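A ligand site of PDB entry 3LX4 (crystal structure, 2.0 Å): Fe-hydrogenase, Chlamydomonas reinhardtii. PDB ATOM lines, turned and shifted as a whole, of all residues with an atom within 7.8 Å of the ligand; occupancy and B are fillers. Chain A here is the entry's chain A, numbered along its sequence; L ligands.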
ATOM      1  N   ALA A  54      -4.785  -3.256  -6.260  1.00  0.00           N
ATOM      2  CA  ALA A  54      -5.635  -2.709  -5.196  1.00  0.00           C
ATOM      3  C   ALA A  54      -4.915  -1.632  -4.370  1.00  0.00           C
ATOM      4  O   ALA A  54      -5.535  -0.682  -3.889  1.00  0.00           O
ATOM      5  CB  ALA A  54      -6.133  -3.823  -4.284  1.00  0.00           C
ATOM      6  N   CYS A 129      -5.831 -18.160  -3.811  1.00  0.00           N
ATOM      7  CA  CYS A 129      -5.069 -16.914  -3.723  1.00  0.00           C
ATOM      8  C   CYS A 129      -5.282 -16.138  -2.423  1.00  0.00           C
ATOM      9  O   CYS A 129      -4.408 -15.378  -2.005  1.00  0.00           O
ATOM     10  CB  CYS A 129      -5.304 -16.010  -4.936  1.00  0.00           C
ATOM     11  SG  CYS A 129      -7.022 -15.684  -5.271  1.00  0.00           S
ATOM     12  N   CYS A 130      -6.425 -16.324  -1.767  1.00  0.00           N
ATOM     13  CA  CYS A 130      -6.687 -15.645  -0.498  1.00  0.00           C
ATOM     14  C   CYS A 130      -6.172 -16.439   0.694  1.00  0.00           C
ATOM     15  O   CYS A 130      -6.660 -17.541   0.957  1.00  0.00           O
ATOM     16  CB  CYS A 130      -8.177 -15.381  -0.318  1.00  0.00           C
ATOM     17  SG  CYS A 130      -8.552 -14.564   1.237  1.00  0.00           S
ATOM     18  N   PRO A 131      -5.164 -15.910   1.412  1.00  0.00           N
ATOM     19  CA  PRO A 131      -4.613 -16.608   2.585  1.00  0.00           C
ATOM     20  C   PRO A 131      -5.602 -16.748   3.735  1.00  0.00           C
ATOM     21  O   PRO A 131      -5.437 -17.634   4.572  1.00  0.00           O
ATOM     22  CB  PRO A 131      -3.416 -15.741   3.003  1.00  0.00           C
ATOM     23  CG  PRO A 131      -3.583 -14.428   2.299  1.00  0.00           C
ATOM     24  CD  PRO A 131      -4.447 -14.651   1.107  1.00  0.00           C
ATOM     25  N   GLY A 132      -6.627 -15.901   3.772  1.00  0.00           N
ATOM     26  CA  GLY A 132      -7.699 -16.013   4.765  1.00  0.00           C
ATOM     27  C   GLY A 132      -8.496 -17.295   4.535  1.00  0.00           C
ATOM     28  O   GLY A 132      -8.826 -18.010   5.483  1.00  0.00           O
ATOM     29  N   TRP A 133      -8.782 -17.575   3.271  1.00  0.00           N
ATOM     30  CA  TRP A 133      -9.439 -18.820   2.889  1.00  0.00           C
ATOM     31  C   TRP A 133      -8.533 -20.024   3.170  1.00  0.00           C
ATOM     32  O   TRP A 133      -8.957 -21.005   3.780  1.00  0.00           O
ATOM     33  CB  TRP A 133      -9.867 -18.769   1.415  1.00  0.00           C
ATOM     34  CG  TRP A 133      -9.988 -20.117   0.716  1.00  0.00           C
ATOM     35  CD1 TRP A 133      -9.345 -20.501  -0.421  1.00  0.00           C
ATOM     36  CD2 TRP A 133     -10.802 -21.231   1.115  1.00  0.00           C
ATOM     37  NE1 TRP A 133      -9.698 -21.785  -0.753  1.00  0.00           N
ATOM     38  CE2 TRP A 133     -10.595 -22.251   0.173  1.00  0.00           C
ATOM     39  CE3 TRP A 133     -11.683 -21.453   2.181  1.00  0.00           C
ATOM     40  CZ2 TRP A 133     -11.234 -23.490   0.263  1.00  0.00           C
ATOM     41  CZ3 TRP A 133     -12.315 -22.687   2.267  1.00  0.00           C
ATOM     42  CH2 TRP A 133     -12.094 -23.681   1.313  1.00  0.00           C
ATOM     43  N   SER A 153      -0.104 -17.873  -5.007  1.00  0.00           N
ATOM     44  CA  SER A 153      -0.694 -16.596  -5.353  1.00  0.00           C
ATOM     45  C   SER A 153       0.176 -15.839  -6.369  1.00  0.00           C
ATOM     46  O   SER A 153       1.358 -16.158  -6.547  1.00  0.00           O
ATOM     47  CB  SER A 153      -0.829 -15.741  -4.100  1.00  0.00           C
ATOM     48  OG  SER A 153       0.460 -15.361  -3.640  1.00  0.00           O
ATOM     49  N   MET A 183       0.734  -4.735  -0.429  1.00  0.00           N
ATOM     50  CA  MET A 183      -0.533  -5.439  -0.525  1.00  0.00           C
ATOM     51  C   MET A 183      -1.634  -4.685   0.226  1.00  0.00           C
ATOM     52  O   MET A 183      -1.351  -3.942   1.167  1.00  0.00           O
ATOM     53  CB  MET A 183      -0.384  -6.851   0.050  1.00  0.00           C
ATOM     54  CG  MET A 183       0.510  -7.762  -0.798  1.00  0.00           C
ATOM     55  SD  MET A 183      -0.367  -8.298  -2.283  1.00  0.00           S
ATOM     56  CE  MET A 183       0.956  -8.280  -3.477  1.00  0.00           C
ATOM     57  N   PRO A 184      -2.901  -4.885  -0.175  1.00  0.00           N
ATOM     58  CA  PRO A 184      -4.049  -4.253   0.486  1.00  0.00           C
ATOM     59  C   PRO A 184      -4.461  -5.069   1.696  1.00  0.00           C
ATOM     60  O   PRO A 184      -5.506  -4.842   2.285  1.00  0.00           O
ATOM     61  CB  PRO A 184      -5.140  -4.337  -0.569  1.00  0.00           C
ATOM     62  CG  PRO A 184      -4.849  -5.646  -1.265  1.00  0.00           C
ATOM     63  CD  PRO A 184      -3.331  -5.735  -1.311  1.00  0.00           C
ATOM     64  N   CYS A 185      -3.596  -6.001   2.061  1.00  0.00           N
ATOM     65  CA  CYS A 185      -4.006  -7.150   2.848  1.00  0.00           C
ATOM     66  C   CYS A 185      -3.071  -7.369   4.032  1.00  0.00           C
ATOM     67  O   CYS A 185      -1.850  -7.361   3.884  1.00  0.00           O
ATOM     68  CB  CYS A 185      -3.995  -8.377   1.930  1.00  0.00           C
ATOM     69  SG  CYS A 185      -4.461  -9.905   2.707  1.00  0.00           S
ATOM     70  N   THR A 186      -3.669  -7.606   5.200  1.00  0.00           N
ATOM     71  CA  THR A 186      -2.900  -7.862   6.413  1.00  0.00           C
ATOM     72  C   THR A 186      -2.484  -9.336   6.556  1.00  0.00           C
ATOM     73  O   THR A 186      -1.732  -9.683   7.475  1.00  0.00           O
ATOM     74  CB  THR A 186      -3.696  -7.421   7.667  1.00  0.00           C
ATOM     75  OG1 THR A 186      -4.910  -8.178   7.765  1.00  0.00           O
ATOM     76  CG2 THR A 186      -4.056  -5.935   7.590  1.00  0.00           C
ATOM     77  N   ARG A 187      -2.946 -10.206   5.664  1.00  0.00           N
ATOM     78  CA  ARG A 187      -2.664 -11.652   5.764  1.00  0.00           C
ATOM     79  C   ARG A 187      -1.566 -12.139   4.802  1.00  0.00           C
ATOM     80  O   ARG A 187      -1.184 -13.317   4.822  1.00  0.00           O
ATOM     81  CB  ARG A 187      -3.927 -12.465   5.513  1.00  0.00           C
ATOM     82  CG  ARG A 187      -5.143 -12.085   6.358  1.00  0.00           C
ATOM     83  CD  ARG A 187      -6.312 -13.005   6.035  1.00  0.00           C
ATOM     84  NE  ARG A 187      -7.619 -12.418   6.345  1.00  0.00           N
ATOM     85  CZ  ARG A 187      -8.483 -12.937   7.223  1.00  0.00           C
ATOM     86  NH1 ARG A 187      -8.177 -14.038   7.885  1.00  0.00           N
ATOM     87  NH2 ARG A 187      -9.653 -12.341   7.434  1.00  0.00           N
ATOM     88  N   LYS A 188      -1.078 -11.244   3.948  1.00  0.00           N
ATOM     89  CA  LYS A 188      -0.130 -11.625   2.902  1.00  0.00           C
ATOM     90  C   LYS A 188       1.268 -11.970   3.427  1.00  0.00           C
ATOM     91  O   LYS A 188       1.982 -12.763   2.817  1.00  0.00           O
ATOM     92  CB  LYS A 188      -0.079 -10.561   1.804  1.00  0.00           C
ATOM     93  CG  LYS A 188      -1.277 -10.654   0.849  1.00  0.00           C
ATOM     94  CD  LYS A 188      -1.184 -11.890  -0.037  1.00  0.00           C
ATOM     95  CE  LYS A 188      -2.482 -12.168  -0.764  1.00  0.00           C
ATOM     96  NZ  LYS A 188      -2.380 -13.382  -1.627  1.00  0.00           N
ATOM     97  N   GLU A 191       1.094 -15.593   4.408  1.00  0.00           N
ATOM     98  CA  GLU A 191       1.253 -16.347   3.172  1.00  0.00           C
ATOM     99  C   GLU A 191       2.731 -16.470   2.801  1.00  0.00           C
ATOM    100  O   GLU A 191       3.236 -17.576   2.566  1.00  0.00           O
ATOM    101  CB  GLU A 191       0.463 -15.697   2.032  1.00  0.00           C
ATOM    102  CG  GLU A 191       0.673 -16.319   0.654  1.00  0.00           C
ATOM    103  CD  GLU A 191      -0.056 -15.534  -0.426  1.00  0.00           C
ATOM    104  OE1 GLU A 191      -1.283 -15.689  -0.560  1.00  0.00           O
ATOM    105  OE2 GLU A 191       0.605 -14.749  -1.137  1.00  0.00           O
ATOM    106  N   ALA A 349     -17.467 -16.506  -3.537  1.00  0.00           N
ATOM    107  CA  ALA A 349     -17.901 -16.198  -2.169  1.00  0.00           C
ATOM    108  C   ALA A 349     -17.066 -15.080  -1.532  1.00  0.00           C
ATOM    109  O   ALA A 349     -15.830 -15.110  -1.585  1.00  0.00           O
ATOM    110  CB  ALA A 349     -17.854 -17.450  -1.306  1.00  0.00           C
ATOM    111  N   ASN A 350     -17.751 -14.104  -0.952  1.00  0.00           N
ATOM    112  CA  ASN A 350     -17.152 -13.052  -0.125  1.00  0.00           C
ATOM    113  C   ASN A 350     -18.047 -12.935   1.125  1.00  0.00           C
ATOM    114  O   ASN A 350     -19.247 -12.776   0.977  1.00  0.00           O
ATOM    115  CB  ASN A 350     -17.205 -11.695  -0.866  1.00  0.00           C
ATOM    116  CG  ASN A 350     -16.454 -11.688  -2.208  1.00  0.00           C
ATOM    117  OD1 ASN A 350     -15.325 -11.189  -2.290  1.00  0.00           O
ATOM    118  ND2 ASN A 350     -17.090 -12.172  -3.260  1.00  0.00           N
ATOM    119  N   GLY A 351     -17.544 -13.050   2.356  1.00  0.00           N
ATOM    120  CA  GLY A 351     -16.228 -13.524   2.716  1.00  0.00           C
ATOM    121  C   GLY A 351     -16.401 -14.811   3.516  1.00  0.00           C
ATOM    122  O   GLY A 351     -17.192 -15.669   3.146  1.00  0.00           O
ATOM    123  N   LEU A 352     -15.691 -14.936   4.643  1.00  0.00           N
ATOM    124  CA  LEU A 352     -15.517 -16.258   5.270  1.00  0.00           C
ATOM    125  C   LEU A 352     -16.767 -16.867   5.934  1.00  0.00           C
ATOM    126  O   LEU A 352     -16.977 -18.072   5.850  1.00  0.00           O
ATOM    127  CB  LEU A 352     -14.324 -16.275   6.228  1.00  0.00           C
ATOM    128  CG  LEU A 352     -12.948 -16.032   5.592  1.00  0.00           C
ATOM    129  CD1 LEU A 352     -11.831 -16.112   6.624  1.00  0.00           C
ATOM    130  CD2 LEU A 352     -12.681 -17.007   4.444  1.00  0.00           C
ATOM    131  N   ILE A 374     -13.102 -18.285  -3.215  1.00  0.00           N
ATOM    132  CA  ILE A 374     -13.404 -17.770  -1.885  1.00  0.00           C
ATOM    133  C   ILE A 374     -12.417 -16.688  -1.490  1.00  0.00           C
ATOM    134  O   ILE A 374     -11.199 -16.903  -1.471  1.00  0.00           O
ATOM    135  CB  ILE A 374     -13.407 -18.900  -0.825  1.00  0.00           C
ATOM    136  CG1 ILE A 374     -14.510 -19.919  -1.128  1.00  0.00           C
ATOM    137  CG2 ILE A 374     -13.572 -18.317   0.573  1.00  0.00           C
ATOM    138  CD1 ILE A 374     -14.361 -21.247  -0.403  1.00  0.00           C
ATOM    139  N   MET A 375     -12.962 -15.508  -1.189  1.00  0.00           N
ATOM    140  CA  MET A 375     -12.203 -14.345  -0.748  1.00  0.00           C
ATOM    141  C   MET A 375     -12.676 -14.002   0.653  1.00  0.00           C
ATOM    142  O   MET A 375     -13.889 -13.906   0.897  1.00  0.00           O
ATOM    143  CB  MET A 375     -12.489 -13.143  -1.654  1.00  0.00           C
ATOM    144  CG  MET A 375     -12.040 -13.283  -3.099  1.00  0.00           C
ATOM    145  SD  MET A 375     -10.253 -13.210  -3.308  1.00  0.00           S
ATOM    146  CE  MET A 375      -9.889 -14.884  -3.764  1.00  0.00           C
ATOM    147  N   ALA A 376     -11.734 -13.802   1.567  1.00  0.00           N
ATOM    148  CA  ALA A 376     -12.068 -13.511   2.963  1.00  0.00           C
ATOM    149  C   ALA A 376     -12.753 -12.152   3.156  1.00  0.00           C
ATOM    150  O   ALA A 376     -13.595 -12.002   4.042  1.00  0.00           O
ATOM    151  CB  ALA A 376     -10.824 -13.606   3.842  1.00  0.00           C
ATOM    152  N   CYS A 377     -12.399 -11.187   2.321  1.00  0.00           N
ATOM    153  CA  CYS A 377     -12.974  -9.840   2.440  1.00  0.00           C
ATOM    154  C   CYS A 377     -14.304  -9.683   1.678  1.00  0.00           C
ATOM    155  O   CYS A 377     -14.404 -10.064   0.518  1.00  0.00           O
ATOM    156  CB  CYS A 377     -11.970  -8.789   1.979  1.00  0.00           C
ATOM    157  SG  CYS A 377     -10.476  -8.741   2.988  1.00  0.00           S
ATOM    158  N   PRO A 378     -15.332  -9.121   2.345  1.00  0.00           N
ATOM    159  CA  PRO A 378     -16.633  -8.854   1.749  1.00  0.00           C
ATOM    160  C   PRO A 378     -16.551  -8.170   0.386  1.00  0.00           C
ATOM    161  O   PRO A 378     -17.272  -8.550  -0.531  1.00  0.00           O
ATOM    162  CB  PRO A 378     -17.284  -7.911   2.774  1.00  0.00           C
ATOM    163  CG  PRO A 378     -16.713  -8.336   4.066  1.00  0.00           C
ATOM    164  CD  PRO A 378     -15.292  -8.756   3.780  1.00  0.00           C
ATOM    165  N   ALA A 379     -15.683  -7.171   0.266  1.00  0.00           N
ATOM    166  CA  ALA A 379     -15.568  -6.414  -0.977  1.00  0.00           C
ATOM    167  C   ALA A 379     -14.414  -6.876  -1.854  1.00  0.00           C
ATOM    168  O   ALA A 379     -14.105  -6.247  -2.868  1.00  0.00           O
ATOM    169  CB  ALA A 379     -15.447  -4.921  -0.669  1.00  0.00           C
ATOM    170  N   GLY A 380     -13.777  -7.978  -1.467  1.00  0.00           N
ATOM    171  CA  GLY A 380     -12.585  -8.439  -2.172  1.00  0.00           C
ATOM    172  C   GLY A 380     -11.375  -7.600  -1.771  1.00  0.00           C
ATOM    173  O   GLY A 380     -11.433  -6.835  -0.798  1.00  0.00           O
ATOM    174  N   CYS A 381     -10.294  -7.724  -2.522  1.00  0.00           N
ATOM    175  CA  CYS A 381      -9.030  -7.117  -2.122  1.00  0.00           C
ATOM    176  C   CYS A 381      -9.051  -5.584  -2.056  1.00  0.00           C
ATOM    177  O   CYS A 381      -8.335  -4.999  -1.243  1.00  0.00           O
ATOM    178  CB  CYS A 381      -7.874  -7.616  -3.000  1.00  0.00           C
ATOM    179  SG  CYS A 381      -7.603  -9.399  -2.818  1.00  0.00           S
ATOM    180  N   VAL A 382      -9.876  -4.951  -2.876  1.00  0.00           N
ATOM    181  CA  VAL A 382      -9.983  -3.494  -2.825  1.00  0.00           C
ATOM    182  C   VAL A 382     -10.496  -3.055  -1.451  1.00  0.00           C
ATOM    183  O   VAL A 382     -10.274  -1.920  -1.044  1.00  0.00           O
ATOM    184  CB  VAL A 382     -10.872  -2.888  -3.954  1.00  0.00           C
ATOM    185  CG1 VAL A 382     -10.222  -3.063  -5.319  1.00  0.00           C
ATOM    186  CG2 VAL A 382     -12.294  -3.470  -3.910  1.00  0.00           C
ATOM    187  N   GLY A 383     -11.175  -3.962  -0.752  1.00  0.00           N
ATOM    188  CA  GLY A 383     -11.640  -3.693   0.604  1.00  0.00           C
ATOM    189  C   GLY A 383     -10.843  -4.406   1.685  1.00  0.00           C
ATOM    190  O   GLY A 383     -11.352  -4.609   2.784  1.00  0.00           O
ATOM    191  N   GLY A 384      -9.604  -4.773   1.384  1.00  0.00           N
ATOM    192  CA  GLY A 384      -8.752  -5.483   2.339  1.00  0.00           C
ATOM    193  C   GLY A 384      -8.388  -4.711   3.595  1.00  0.00           C
ATOM    194  O   GLY A 384      -8.489  -3.486   3.637  1.00  0.00           O
ATOM    195  N   GLY A 385      -7.952  -5.435   4.626  1.00  0.00           N
ATOM    196  CA  GLY A 385      -7.691  -4.857   5.939  1.00  0.00           C
ATOM    197  C   GLY A 385      -6.519  -3.891   6.030  1.00  0.00           C
ATOM    198  O   GLY A 385      -6.398  -3.155   7.001  1.00  0.00           O
ATOM    199  N   GLY A 386      -5.654  -3.906   5.008  1.00  0.00           N
ATOM    200  CA  GLY A 386      -4.525  -2.982   4.961  1.00  0.00           C
ATOM    201  C   GLY A 386      -4.829  -1.697   4.199  1.00  0.00           C
ATOM    202  O   GLY A 386      -3.946  -0.859   4.014  1.00  0.00           O
ATOM    203  N   GLN A 387      -6.075  -1.535   3.770  1.00  0.00           N
ATOM    204  CA  GLN A 387      -6.480  -0.379   2.990  1.00  0.00           C
ATOM    205  C   GLN A 387      -6.832   0.818   3.890  1.00  0.00           C
ATOM    206  O   GLN A 387      -7.132   0.641   5.070  1.00  0.00           O
ATOM    207  CB  GLN A 387      -7.700  -0.727   2.119  1.00  0.00           C
ATOM    208  CG  GLN A 387      -7.450  -1.755   1.013  1.00  0.00           C
ATOM    209  CD  GLN A 387      -6.638  -1.212  -0.150  1.00  0.00           C
ATOM    210  OE1 GLN A 387      -5.512  -0.746   0.019  1.00  0.00           O
ATOM    211  NE2 GLN A 387      -7.209  -1.300  -1.352  1.00  0.00           N
HETATM  212 FE1  LIG L   1      -8.141 -12.352   0.913  1.00  0.00          FE
HETATM  213 FE2  LIG L   1      -8.907  -9.859   1.811  1.00  0.00          FE
HETATM  214 FE3  LIG L   1      -6.309 -10.476   1.573  1.00  0.00          FE
HETATM  215 FE4  LIG L   1      -7.780 -10.138  -0.691  1.00  0.00          FE
HETATM  216  S1  LIG L   1      -7.284  -8.513   0.866  1.00  0.00           S
HETATM  217  S2  LIG L   1      -6.270 -11.834  -0.305  1.00  0.00           S
HETATM  218  S3  LIG L   1      -9.792 -11.009   0.023  1.00  0.00           S
HETATM  219  S4  LIG L   1      -7.805 -11.468   3.025  1.00  0.00           S
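The side-chain sulfur (SG) of Cys 185 sits close to the backbone NH (N) of Arg 187 (3.3 Å).
The backbone carbonyl oxygen (O) of Cys 377 sits close to the side-chain amide oxygen (OD1) of Asn 350, 3.2 Å away.
The side-chain sulfur of Cys 130 sits close to the backbone NH of Ala 376.
The backbone NH (N) of Gly 132 sits close to the side-chain sulfur (SG) of Cys 130 (3.5 Å).
SG of Cys 130 sits close to N of Trp 133, 3.6 Å away.
O of Ala 349 is in hydrogen-bond range of N of Met 375, 2.9 Å away.
The side-chain amino group of Lys 188 lies within hydrogen-bond range of the backbone carbonyl oxygen of Cys 129, at 2.9 Å.
NZ of Lys 188 lies within salt-bridge range of OE1 of Glu 191.
Merely in contact with the ligand: Pro 131 (3.6 Å), Gly 384 (3.7 Å), Met 375 (3.8 Å) and Lys 188 (3.8 Å).
Ten residues have an atom within 4 Å of the ligand: Cys 130, Pro 131, Cys 185, Arg 187, Lys 188, Met 375, Ala 376, Cys 377, Cys 381 and Gly 384.
The side-chain sulfur (SG) of Cys 185 binds an iron atom (FE3) of the ligand (2.2 Å).
The backbone NH of Cys 377 sits close to a sulfur (S3) of the ligand (3.5 Å).
The side-chain sulfur of Cys 377 binds an iron atom (FE2) of the ligand, at 2.3 Å.
The side-chain sulfur (SG) of Cys 381 binds an iron atom (FE4) of the ligand, 2.3 Å away.
The side-chain sulfur (SG) of Cys 130 is bound to an iron atom (FE1) of the ligand.
NE of Arg 187 lies close to S4 of the ligand.
The backbone NH (N) of Ala 376 lies close to a sulfur (S3) of the ligand, at 3.7 Å.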
